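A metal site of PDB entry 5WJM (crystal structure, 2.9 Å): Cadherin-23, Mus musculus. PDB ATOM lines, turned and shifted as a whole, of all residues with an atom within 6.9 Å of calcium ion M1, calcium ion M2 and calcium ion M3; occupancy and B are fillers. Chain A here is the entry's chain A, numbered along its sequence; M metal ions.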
ATOM      1  N   GLU A  19      16.505  32.399  -7.909  1.00  0.00           N
ATOM      2  CA  GLU A  19      16.350  32.924  -9.261  1.00  0.00           C
ATOM      3  C   GLU A  19      14.868  32.893  -9.666  1.00  0.00           C
ATOM      4  O   GLU A  19      14.081  32.113  -9.135  1.00  0.00           O
ATOM      5  CB  GLU A  19      17.242  32.178 -10.292  1.00  0.00           C
ATOM      6  CG  GLU A  19      16.946  30.690 -10.511  1.00  0.00           C
ATOM      7  CD  GLU A  19      17.596  30.073 -11.764  1.00  0.00           C
ATOM      8  OE1 GLU A  19      17.962  30.753 -12.741  1.00  0.00           O
ATOM      9  OE2 GLU A  19      17.743  28.839 -11.782  1.00  0.00           O
ATOM     10  N   GLY A  20      14.501  33.783 -10.586  1.00  0.00           N
ATOM     11  CA  GLY A  20      13.126  33.819 -11.143  1.00  0.00           C
ATOM     12  C   GLY A  20      12.106  34.544 -10.277  1.00  0.00           C
ATOM     13  O   GLY A  20      10.919  34.588 -10.612  1.00  0.00           O
ATOM     14  N   LEU A  72      16.587  37.563 -10.634  1.00  0.00           N
ATOM     15  CA  LEU A  72      17.950  37.036 -10.770  1.00  0.00           C
ATOM     16  C   LEU A  72      17.962  35.730 -11.619  1.00  0.00           C
ATOM     17  O   LEU A  72      16.922  35.108 -11.804  1.00  0.00           O
ATOM     18  CB  LEU A  72      18.584  36.807  -9.394  1.00  0.00           C
ATOM     19  CG  LEU A  72      18.737  38.007  -8.458  1.00  0.00           C
ATOM     20  CD1 LEU A  72      19.371  37.590  -7.148  1.00  0.00           C
ATOM     21  CD2 LEU A  72      19.596  39.094  -9.062  1.00  0.00           C
ATOM     22  N   ASP A  73      19.149  35.356 -12.118  1.00  0.00           N
ATOM     23  CA  ASP A  73      19.370  34.150 -12.950  1.00  0.00           C
ATOM     24  C   ASP A  73      20.715  33.477 -12.601  1.00  0.00           C
ATOM     25  O   ASP A  73      21.777  33.977 -12.934  1.00  0.00           O
ATOM     26  CB  ASP A  73      19.322  34.537 -14.432  1.00  0.00           C
ATOM     27  CG  ASP A  73      19.763  33.383 -15.387  1.00  0.00           C
ATOM     28  OD1 ASP A  73      19.414  32.188 -15.138  1.00  0.00           O
ATOM     29  OD2 ASP A  73      20.448  33.673 -16.406  1.00  0.00           O
ATOM     30  N   ARG A  74      20.649  32.318 -11.957  1.00  0.00           N
ATOM     31  CA  ARG A  74      21.844  31.589 -11.518  1.00  0.00           C
ATOM     32  C   ARG A  74      22.805  31.178 -12.630  1.00  0.00           C
ATOM     33  O   ARG A  74      24.031  31.088 -12.427  1.00  0.00           O
ATOM     34  CB  ARG A  74      21.426  30.344 -10.769  1.00  0.00           C
ATOM     35  CG  ARG A  74      22.519  29.776  -9.895  1.00  0.00           C
ATOM     36  CD  ARG A  74      22.127  28.403  -9.418  1.00  0.00           C
ATOM     37  NE  ARG A  74      22.053  27.517 -10.583  1.00  0.00           N
ATOM     38  CZ  ARG A  74      23.078  26.874 -11.133  1.00  0.00           C
ATOM     39  NH1 ARG A  74      24.295  26.939 -10.606  1.00  0.00           N
ATOM     40  NH2 ARG A  74      22.883  26.130 -12.201  1.00  0.00           N
ATOM     41  N   GLU A  75      22.258  30.883 -13.810  1.00  0.00           N
ATOM     42  CA  GLU A  75      23.076  30.458 -14.958  1.00  0.00           C
ATOM     43  C   GLU A  75      23.942  31.600 -15.595  1.00  0.00           C
ATOM     44  O   GLU A  75      24.897  31.297 -16.338  1.00  0.00           O
ATOM     45  CB  GLU A  75      22.189  29.798 -16.033  1.00  0.00           C
ATOM     46  CG  GLU A  75      21.663  28.408 -15.674  1.00  0.00           C
ATOM     47  CD  GLU A  75      20.463  28.384 -14.713  1.00  0.00           C
ATOM     48  OE1 GLU A  75      20.522  27.592 -13.742  1.00  0.00           O
ATOM     49  OE2 GLU A  75      19.442  29.097 -14.918  1.00  0.00           O
ATOM     50  N   THR A  76      23.621  32.902 -15.325  1.00  0.00           N
ATOM     51  CA  THR A  76      24.494  34.013 -15.737  1.00  0.00           C
ATOM     52  C   THR A  76      25.325  34.505 -14.547  1.00  0.00           C
ATOM     53  O   THR A  76      26.529  34.712 -14.678  1.00  0.00           O
ATOM     54  CB  THR A  76      23.757  35.171 -16.466  1.00  0.00           C
ATOM     55  OG1 THR A  76      22.702  35.655 -15.670  1.00  0.00           O
ATOM     56  CG2 THR A  76      23.163  34.728 -17.833  1.00  0.00           C
ATOM     57  N   LEU A 105      20.084  30.935  -5.364  1.00  0.00           N
ATOM     58  CA  LEU A 105      19.562  29.564  -5.284  1.00  0.00           C
ATOM     59  C   LEU A 105      18.885  29.159  -6.596  1.00  0.00           C
ATOM     60  O   LEU A 105      18.105  29.933  -7.176  1.00  0.00           O
ATOM     61  CB  LEU A 105      18.539  29.401  -4.157  1.00  0.00           C
ATOM     62  CG  LEU A 105      18.948  29.530  -2.682  1.00  0.00           C
ATOM     63  CD1 LEU A 105      17.676  29.447  -1.824  1.00  0.00           C
ATOM     64  CD2 LEU A 105      19.980  28.507  -2.228  1.00  0.00           C
ATOM     65  N   ASP A 106      19.164  27.926  -7.018  1.00  0.00           N
ATOM     66  CA  ASP A 106      18.762  27.399  -8.328  1.00  0.00           C
ATOM     67  C   ASP A 106      17.288  27.034  -8.379  1.00  0.00           C
ATOM     68  O   ASP A 106      16.788  26.489  -7.432  1.00  0.00           O
ATOM     69  CB  ASP A 106      19.567  26.130  -8.588  1.00  0.00           C
ATOM     70  CG  ASP A 106      19.314  25.547  -9.939  1.00  0.00           C
ATOM     71  OD1 ASP A 106      19.381  26.297 -10.932  1.00  0.00           O
ATOM     72  OD2 ASP A 106      19.090  24.324 -10.026  1.00  0.00           O
ATOM     73  N   ILE A 107      16.605  27.312  -9.489  1.00  0.00           N
ATOM     74  CA  ILE A 107      15.331  26.632  -9.781  1.00  0.00           C
ATOM     75  C   ILE A 107      15.549  25.757 -11.012  1.00  0.00           C
ATOM     76  O   ILE A 107      16.606  25.864 -11.657  1.00  0.00           O
ATOM     77  CB  ILE A 107      14.118  27.592  -9.962  1.00  0.00           C
ATOM     78  CG1 ILE A 107      14.120  28.285 -11.338  1.00  0.00           C
ATOM     79  CG2 ILE A 107      14.042  28.580  -8.800  1.00  0.00           C
ATOM     80  CD1 ILE A 107      13.059  29.354 -11.517  1.00  0.00           C
ATOM     81  N   ASN A 108      14.572  24.900 -11.320  1.00  0.00           N
ATOM     82  CA  ASN A 108      14.674  24.004 -12.470  1.00  0.00           C
ATOM     83  C   ASN A 108      14.081  24.668 -13.712  1.00  0.00           C
ATOM     84  O   ASN A 108      12.913  24.494 -14.058  1.00  0.00           O
ATOM     85  CB  ASN A 108      13.999  22.670 -12.172  1.00  0.00           C
ATOM     86  CG  ASN A 108      14.348  21.599 -13.194  1.00  0.00           C
ATOM     87  OD1 ASN A 108      15.501  21.477 -13.621  1.00  0.00           O
ATOM     88  ND2 ASN A 108      13.351  20.822 -13.588  1.00  0.00           N
ATOM     89  N   ASP A 109      14.907  25.445 -14.376  1.00  0.00           N
ATOM     90  CA  ASP A 109      14.478  26.260 -15.475  1.00  0.00           C
ATOM     91  C   ASP A 109      15.240  25.909 -16.758  1.00  0.00           C
ATOM     92  O   ASP A 109      15.272  26.705 -17.708  1.00  0.00           O
ATOM     93  CB  ASP A 109      14.565  27.769 -15.088  1.00  0.00           C
ATOM     94  CG  ASP A 109      15.986  28.258 -14.722  1.00  0.00           C
ATOM     95  OD1 ASP A 109      16.706  27.577 -13.963  1.00  0.00           O
ATOM     96  OD2 ASP A 109      16.405  29.336 -15.195  1.00  0.00           O
ATOM     97  N   ASN A 110      15.831  24.712 -16.786  1.00  0.00           N
ATOM     98  CA  ASN A 110      16.594  24.225 -17.940  1.00  0.00           C
ATOM     99  C   ASN A 110      16.281  22.735 -18.178  1.00  0.00           C
ATOM    100  O   ASN A 110      16.465  21.901 -17.280  1.00  0.00           O
ATOM    101  CB  ASN A 110      18.101  24.385 -17.751  1.00  0.00           C
ATOM    102  CG  ASN A 110      18.553  25.841 -17.663  1.00  0.00           C
ATOM    103  OD1 ASN A 110      19.050  26.409 -18.639  1.00  0.00           O
ATOM    104  ND2 ASN A 110      18.435  26.436 -16.484  1.00  0.00           N
ATOM    105  N   ASP A 111      15.827  22.427 -19.387  1.00  0.00           N
ATOM    106  CA  ASP A 111      15.589  21.051 -19.823  1.00  0.00           C
ATOM    107  C   ASP A 111      16.904  20.275 -19.849  1.00  0.00           C
ATOM    108  O   ASP A 111      17.958  20.849 -20.146  1.00  0.00           O
ATOM    109  CB  ASP A 111      14.936  21.020 -21.234  1.00  0.00           C
ATOM    110  CG  ASP A 111      13.444  21.448 -21.238  1.00  0.00           C
ATOM    111  OD1 ASP A 111      12.828  21.615 -20.166  1.00  0.00           O
ATOM    112  OD2 ASP A 111      12.866  21.610 -22.355  1.00  0.00           O
ATOM    113  N   PRO A 112      16.880  18.967 -19.545  1.00  0.00           N
ATOM    114  CA  PRO A 112      18.061  18.175 -19.894  1.00  0.00           C
ATOM    115  C   PRO A 112      18.159  18.059 -21.402  1.00  0.00           C
ATOM    116  O   PRO A 112      17.164  18.263 -22.081  1.00  0.00           O
ATOM    117  CB  PRO A 112      17.794  16.805 -19.229  1.00  0.00           C
ATOM    118  CG  PRO A 112      16.337  16.758 -18.991  1.00  0.00           C
ATOM    119  CD  PRO A 112      15.851  18.166 -18.859  1.00  0.00           C
ATOM    120  N   ASP A 140      22.736  19.119 -18.333  1.00  0.00           N
ATOM    121  CA  ASP A 140      21.691  19.981 -17.721  1.00  0.00           C
ATOM    122  C   ASP A 140      22.371  21.217 -17.076  1.00  0.00           C
ATOM    123  O   ASP A 140      23.288  21.099 -16.256  1.00  0.00           O
ATOM    124  CB  ASP A 140      20.870  19.186 -16.700  1.00  0.00           C
ATOM    125  CG  ASP A 140      19.520  19.849 -16.332  1.00  0.00           C
ATOM    126  OD1 ASP A 140      19.501  20.980 -15.788  1.00  0.00           O
ATOM    127  OD2 ASP A 140      18.460  19.224 -16.549  1.00  0.00           O
ATOM    128  N   ALA A 141      21.911  22.387 -17.459  1.00  0.00           N
ATOM    129  CA  ALA A 141      22.547  23.640 -17.059  1.00  0.00           C
ATOM    130  C   ALA A 141      22.307  24.024 -15.586  1.00  0.00           C
ATOM    131  O   ALA A 141      23.032  24.864 -15.039  1.00  0.00           O
ATOM    132  CB  ALA A 141      22.105  24.769 -17.992  1.00  0.00           C
ATOM    133  N   ASP A 142      21.290  23.408 -14.953  1.00  0.00           N
ATOM    134  CA  ASP A 142      20.951  23.657 -13.545  1.00  0.00           C
ATOM    135  C   ASP A 142      22.033  23.039 -12.630  1.00  0.00           C
ATOM    136  O   ASP A 142      23.044  22.511 -13.123  1.00  0.00           O
ATOM    137  CB  ASP A 142      19.538  23.124 -13.218  1.00  0.00           C
ATOM    138  CG  ASP A 142      18.411  23.821 -14.052  1.00  0.00           C
ATOM    139  OD1 ASP A 142      18.388  25.072 -14.160  1.00  0.00           O
ATOM    140  OD2 ASP A 142      17.535  23.107 -14.617  1.00  0.00           O
ATOM    141  N   SER A 143      21.843  23.157 -11.326  1.00  0.00           N
ATOM    142  CA  SER A 143      22.736  22.559 -10.336  1.00  0.00           C
ATOM    143  C   SER A 143      21.951  21.642  -9.422  1.00  0.00           C
ATOM    144  O   SER A 143      20.710  21.599  -9.492  1.00  0.00           O
ATOM    145  CB  SER A 143      23.416  23.647  -9.504  1.00  0.00           C
ATOM    146  OG  SER A 143      22.552  24.076  -8.454  1.00  0.00           O
ATOM    147  N   CYS A 145      20.030  18.724  -7.420  1.00  0.00           N
ATOM    148  CA  CYS A 145      19.019  17.751  -7.854  1.00  0.00           C
ATOM    149  C   CYS A 145      18.332  18.159  -9.180  1.00  0.00           C
ATOM    150  O   CYS A 145      17.779  17.315  -9.907  1.00  0.00           O
ATOM    151  CB  CYS A 145      17.982  17.527  -6.743  1.00  0.00           C
ATOM    152  SG  CYS A 145      16.836  18.883  -6.439  1.00  0.00           S
ATOM    153  N   ASN A 146      18.385  19.454  -9.527  1.00  0.00           N
ATOM    154  CA  ASN A 146      17.807  19.957 -10.795  1.00  0.00           C
ATOM    155  C   ASN A 146      18.619  19.608 -12.047  1.00  0.00           C
ATOM    156  O   ASN A 146      18.159  19.868 -13.168  1.00  0.00           O
ATOM    157  CB  ASN A 146      17.626  21.490 -10.736  1.00  0.00           C
ATOM    158  CG  ASN A 146      16.678  21.927  -9.636  1.00  0.00           C
ATOM    159  OD1 ASN A 146      15.733  21.231  -9.302  1.00  0.00           O
ATOM    160  ND2 ASN A 146      16.916  23.097  -9.076  1.00  0.00           N
ATOM    161  N   ALA A 147      19.826  19.093 -11.860  1.00  0.00           N
ATOM    162  CA  ALA A 147      20.639  18.574 -12.960  1.00  0.00           C
ATOM    163  C   ALA A 147      21.059  17.111 -12.752  1.00  0.00           C
ATOM    164  O   ALA A 147      21.876  16.597 -13.511  1.00  0.00           O
ATOM    165  CB  ALA A 147      21.862  19.459 -13.180  1.00  0.00           C
ATOM    166  N   LEU A 148      20.459  16.431 -11.769  1.00  0.00           N
ATOM    167  CA  LEU A 148      20.713  15.003 -11.551  1.00  0.00           C
ATOM    168  C   LEU A 148      19.821  14.236 -12.518  1.00  0.00           C
ATOM    169  O   LEU A 148      18.588  14.270 -12.382  1.00  0.00           O
ATOM    170  CB  LEU A 148      20.384  14.603 -10.098  1.00  0.00           C
ATOM    171  CG  LEU A 148      20.403  13.081  -9.812  1.00  0.00           C
ATOM    172  CD1 LEU A 148      21.777  12.498 -10.108  1.00  0.00           C
ATOM    173  CD2 LEU A 148      19.965  12.750  -8.386  1.00  0.00           C
ATOM    174  N   LEU A 149      20.434  13.534 -13.489  1.00  0.00           N
ATOM    175  CA  LEU A 149      19.691  12.923 -14.601  1.00  0.00           C
ATOM    176  C   LEU A 149      19.430  11.422 -14.442  1.00  0.00           C
ATOM    177  O   LEU A 149      20.297  10.675 -13.972  1.00  0.00           O
ATOM    178  CB  LEU A 149      20.431  13.177 -15.916  1.00  0.00           C
ATOM    179  CG  LEU A 149      20.741  14.629 -16.238  1.00  0.00           C
ATOM    180  CD1 LEU A 149      21.298  14.753 -17.642  1.00  0.00           C
ATOM    181  CD2 LEU A 149      19.511  15.490 -16.069  1.00  0.00           C
ATOM    182  N   ASP A 193      15.416  15.152 -15.414  1.00  0.00           N
ATOM    183  CA  ASP A 193      16.000  15.617 -14.154  1.00  0.00           C
ATOM    184  C   ASP A 193      15.077  15.231 -12.978  1.00  0.00           C
ATOM    185  O   ASP A 193      13.964  14.737 -13.165  1.00  0.00           O
ATOM    186  CB  ASP A 193      16.409  17.120 -14.153  1.00  0.00           C
ATOM    187  CG  ASP A 193      15.312  18.060 -14.668  1.00  0.00           C
ATOM    188  OD1 ASP A 193      14.117  17.778 -14.471  1.00  0.00           O
ATOM    189  OD2 ASP A 193      15.649  19.096 -15.272  1.00  0.00           O
ATOM    190  N   ASN A 194      15.596  15.433 -11.773  1.00  0.00           N
ATOM    191  CA  ASN A 194      14.945  14.954 -10.551  1.00  0.00           C
ATOM    192  C   ASN A 194      14.907  16.068  -9.520  1.00  0.00           C
ATOM    193  O   ASN A 194      15.582  15.982  -8.503  1.00  0.00           O
ATOM    194  CB  ASN A 194      15.700  13.730  -9.999  1.00  0.00           C
ATOM    195  CG  ASN A 194      15.681  12.565 -10.955  1.00  0.00           C
ATOM    196  OD1 ASN A 194      14.841  11.690 -10.852  1.00  0.00           O
ATOM    197  ND2 ASN A 194      16.601  12.563 -11.912  1.00  0.00           N
ATOM    198  N   PRO A 195      14.099  17.117  -9.761  1.00  0.00           N
ATOM    199  CA  PRO A 195      13.963  18.184  -8.777  1.00  0.00           C
ATOM    200  C   PRO A 195      13.248  17.687  -7.531  1.00  0.00           C
ATOM    201  O   PRO A 195      12.648  16.626  -7.575  1.00  0.00           O
ATOM    202  CB  PRO A 195      13.130  19.248  -9.508  1.00  0.00           C
ATOM    203  CG  PRO A 195      12.439  18.535 -10.607  1.00  0.00           C
ATOM    204  CD  PRO A 195      13.244  17.312 -10.949  1.00  0.00           C
ATOM    205  N   ARG A 202      11.718  18.160 -15.852  1.00  0.00           N
ATOM    206  CA  ARG A 202      11.824  18.380 -17.301  1.00  0.00           C
ATOM    207  C   ARG A 202      12.555  17.199 -17.954  1.00  0.00           C
ATOM    208  O   ARG A 202      13.355  16.528 -17.296  1.00  0.00           O
ATOM    209  CB  ARG A 202      12.535  19.703 -17.564  1.00  0.00           C
ATOM    210  CG  ARG A 202      12.037  20.859 -16.698  1.00  0.00           C
ATOM    211  CD  ARG A 202      13.009  22.027 -16.611  1.00  0.00           C
ATOM    212  NE  ARG A 202      12.691  23.026 -17.635  1.00  0.00           N
ATOM    213  CZ  ARG A 202      11.848  24.049 -17.480  1.00  0.00           C
ATOM    214  NH1 ARG A 202      11.233  24.268 -16.316  1.00  0.00           N
ATOM    215  NH2 ARG A 202      11.626  24.871 -18.499  1.00  0.00           N
HETATM  216 CA    CA M   1      18.516  26.940 -12.790  1.00  0.00          CA
HETATM  217 CA    CA M   2      17.844  30.797 -15.039  1.00  0.00          CA
HETATM  218 CA    CA M   3      17.202  20.952 -15.130  1.00  0.00          CA
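Calcium ion M1 is bound by the side-chain carboxylate of Asp 106 (2.1 Å), the side-chain carboxylate of Asp 109 (2.2 Å), the side-chain carboxylate of Glu 19 (2.3 Å), the side-chain carboxylate of Glu 75 (2.3 Å), the side-chain carboxylate of Asp 142 (2.3 Å) and the backbone carbonyl oxygen of Ile 107 (2.5 Å).
Calcium ion M1 has six donor atoms within binding distance.
The side-chain amide nitrogen of Asn 110 sits close to the side-chain carboxylate of Asp 109.
ND2 of Asn 146 sits at hydrogen-bond distance from OD2 of Asp 106.
OD1 of Asp 106 sits close to NE of Arg 74 (3.0 Å).
The backbone NH (N) of Arg 74 sits close to the side-chain carboxylate (OE1) of Glu 19, at 3.2 Å.
The backbone carbonyl oxygen of Leu 105 is in hydrogen-bond range of the backbone NH of Glu 19 (3.0 Å).
OE1 of Glu 75 lies close to NH2 of Arg 74 (3.2 Å).
The backbone carbonyl oxygen (O) of Asn 108 is in hydrogen-bond range of the guanidinium group (NH1) of Arg 202, 2.8 Å away.
The side-chain carboxylate (OD1) of Asp 193 lies within hydrogen-bond range of the backbone NH (N) of Arg 202 (2.8 Å).
Within 4 Å of calcium ion M1: Glu 19, Glu 75, Asp 106, Ile 107, Asp 109, Asn 110 and Asp 142.
The nearest printed residue that does not touch calcium ion M1 is Arg 74 (4.2 Å).
Within 4 Å of calcium ion M3: Asn 108, Asn 110, Asp 140, Asp 142, Asn 146 and Asp 193.
The nearest printed residue that does not touch calcium ion M3 is Arg 202 (4.6 Å).
Calcium ion M2 is bound by OD2 of Asp 109, OD1 of Asp 73, OE1 of Glu 19 and OE2 of Glu 75.
The side-chain carboxylate (OD2) of Asp 142 binds calcium ion M3 (2.2 Å).
OD1 of Asn 108 binds calcium ion M3 (2.3 Å).
Calcium ion M3 is bound by OD1 of Asp 140, 2.4 Å away.
Calcium ion M3 is bound by OD2 of Asp 193 (2.4 Å).
O of Asn 146 is bound to calcium ion M3 (2.4 Å).
The backbone carbonyl oxygen (O) of Asn 110 is bound to calcium ion M3.
OD2 of Asp 140 binds calcium ion M3, 2.6 Å away.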
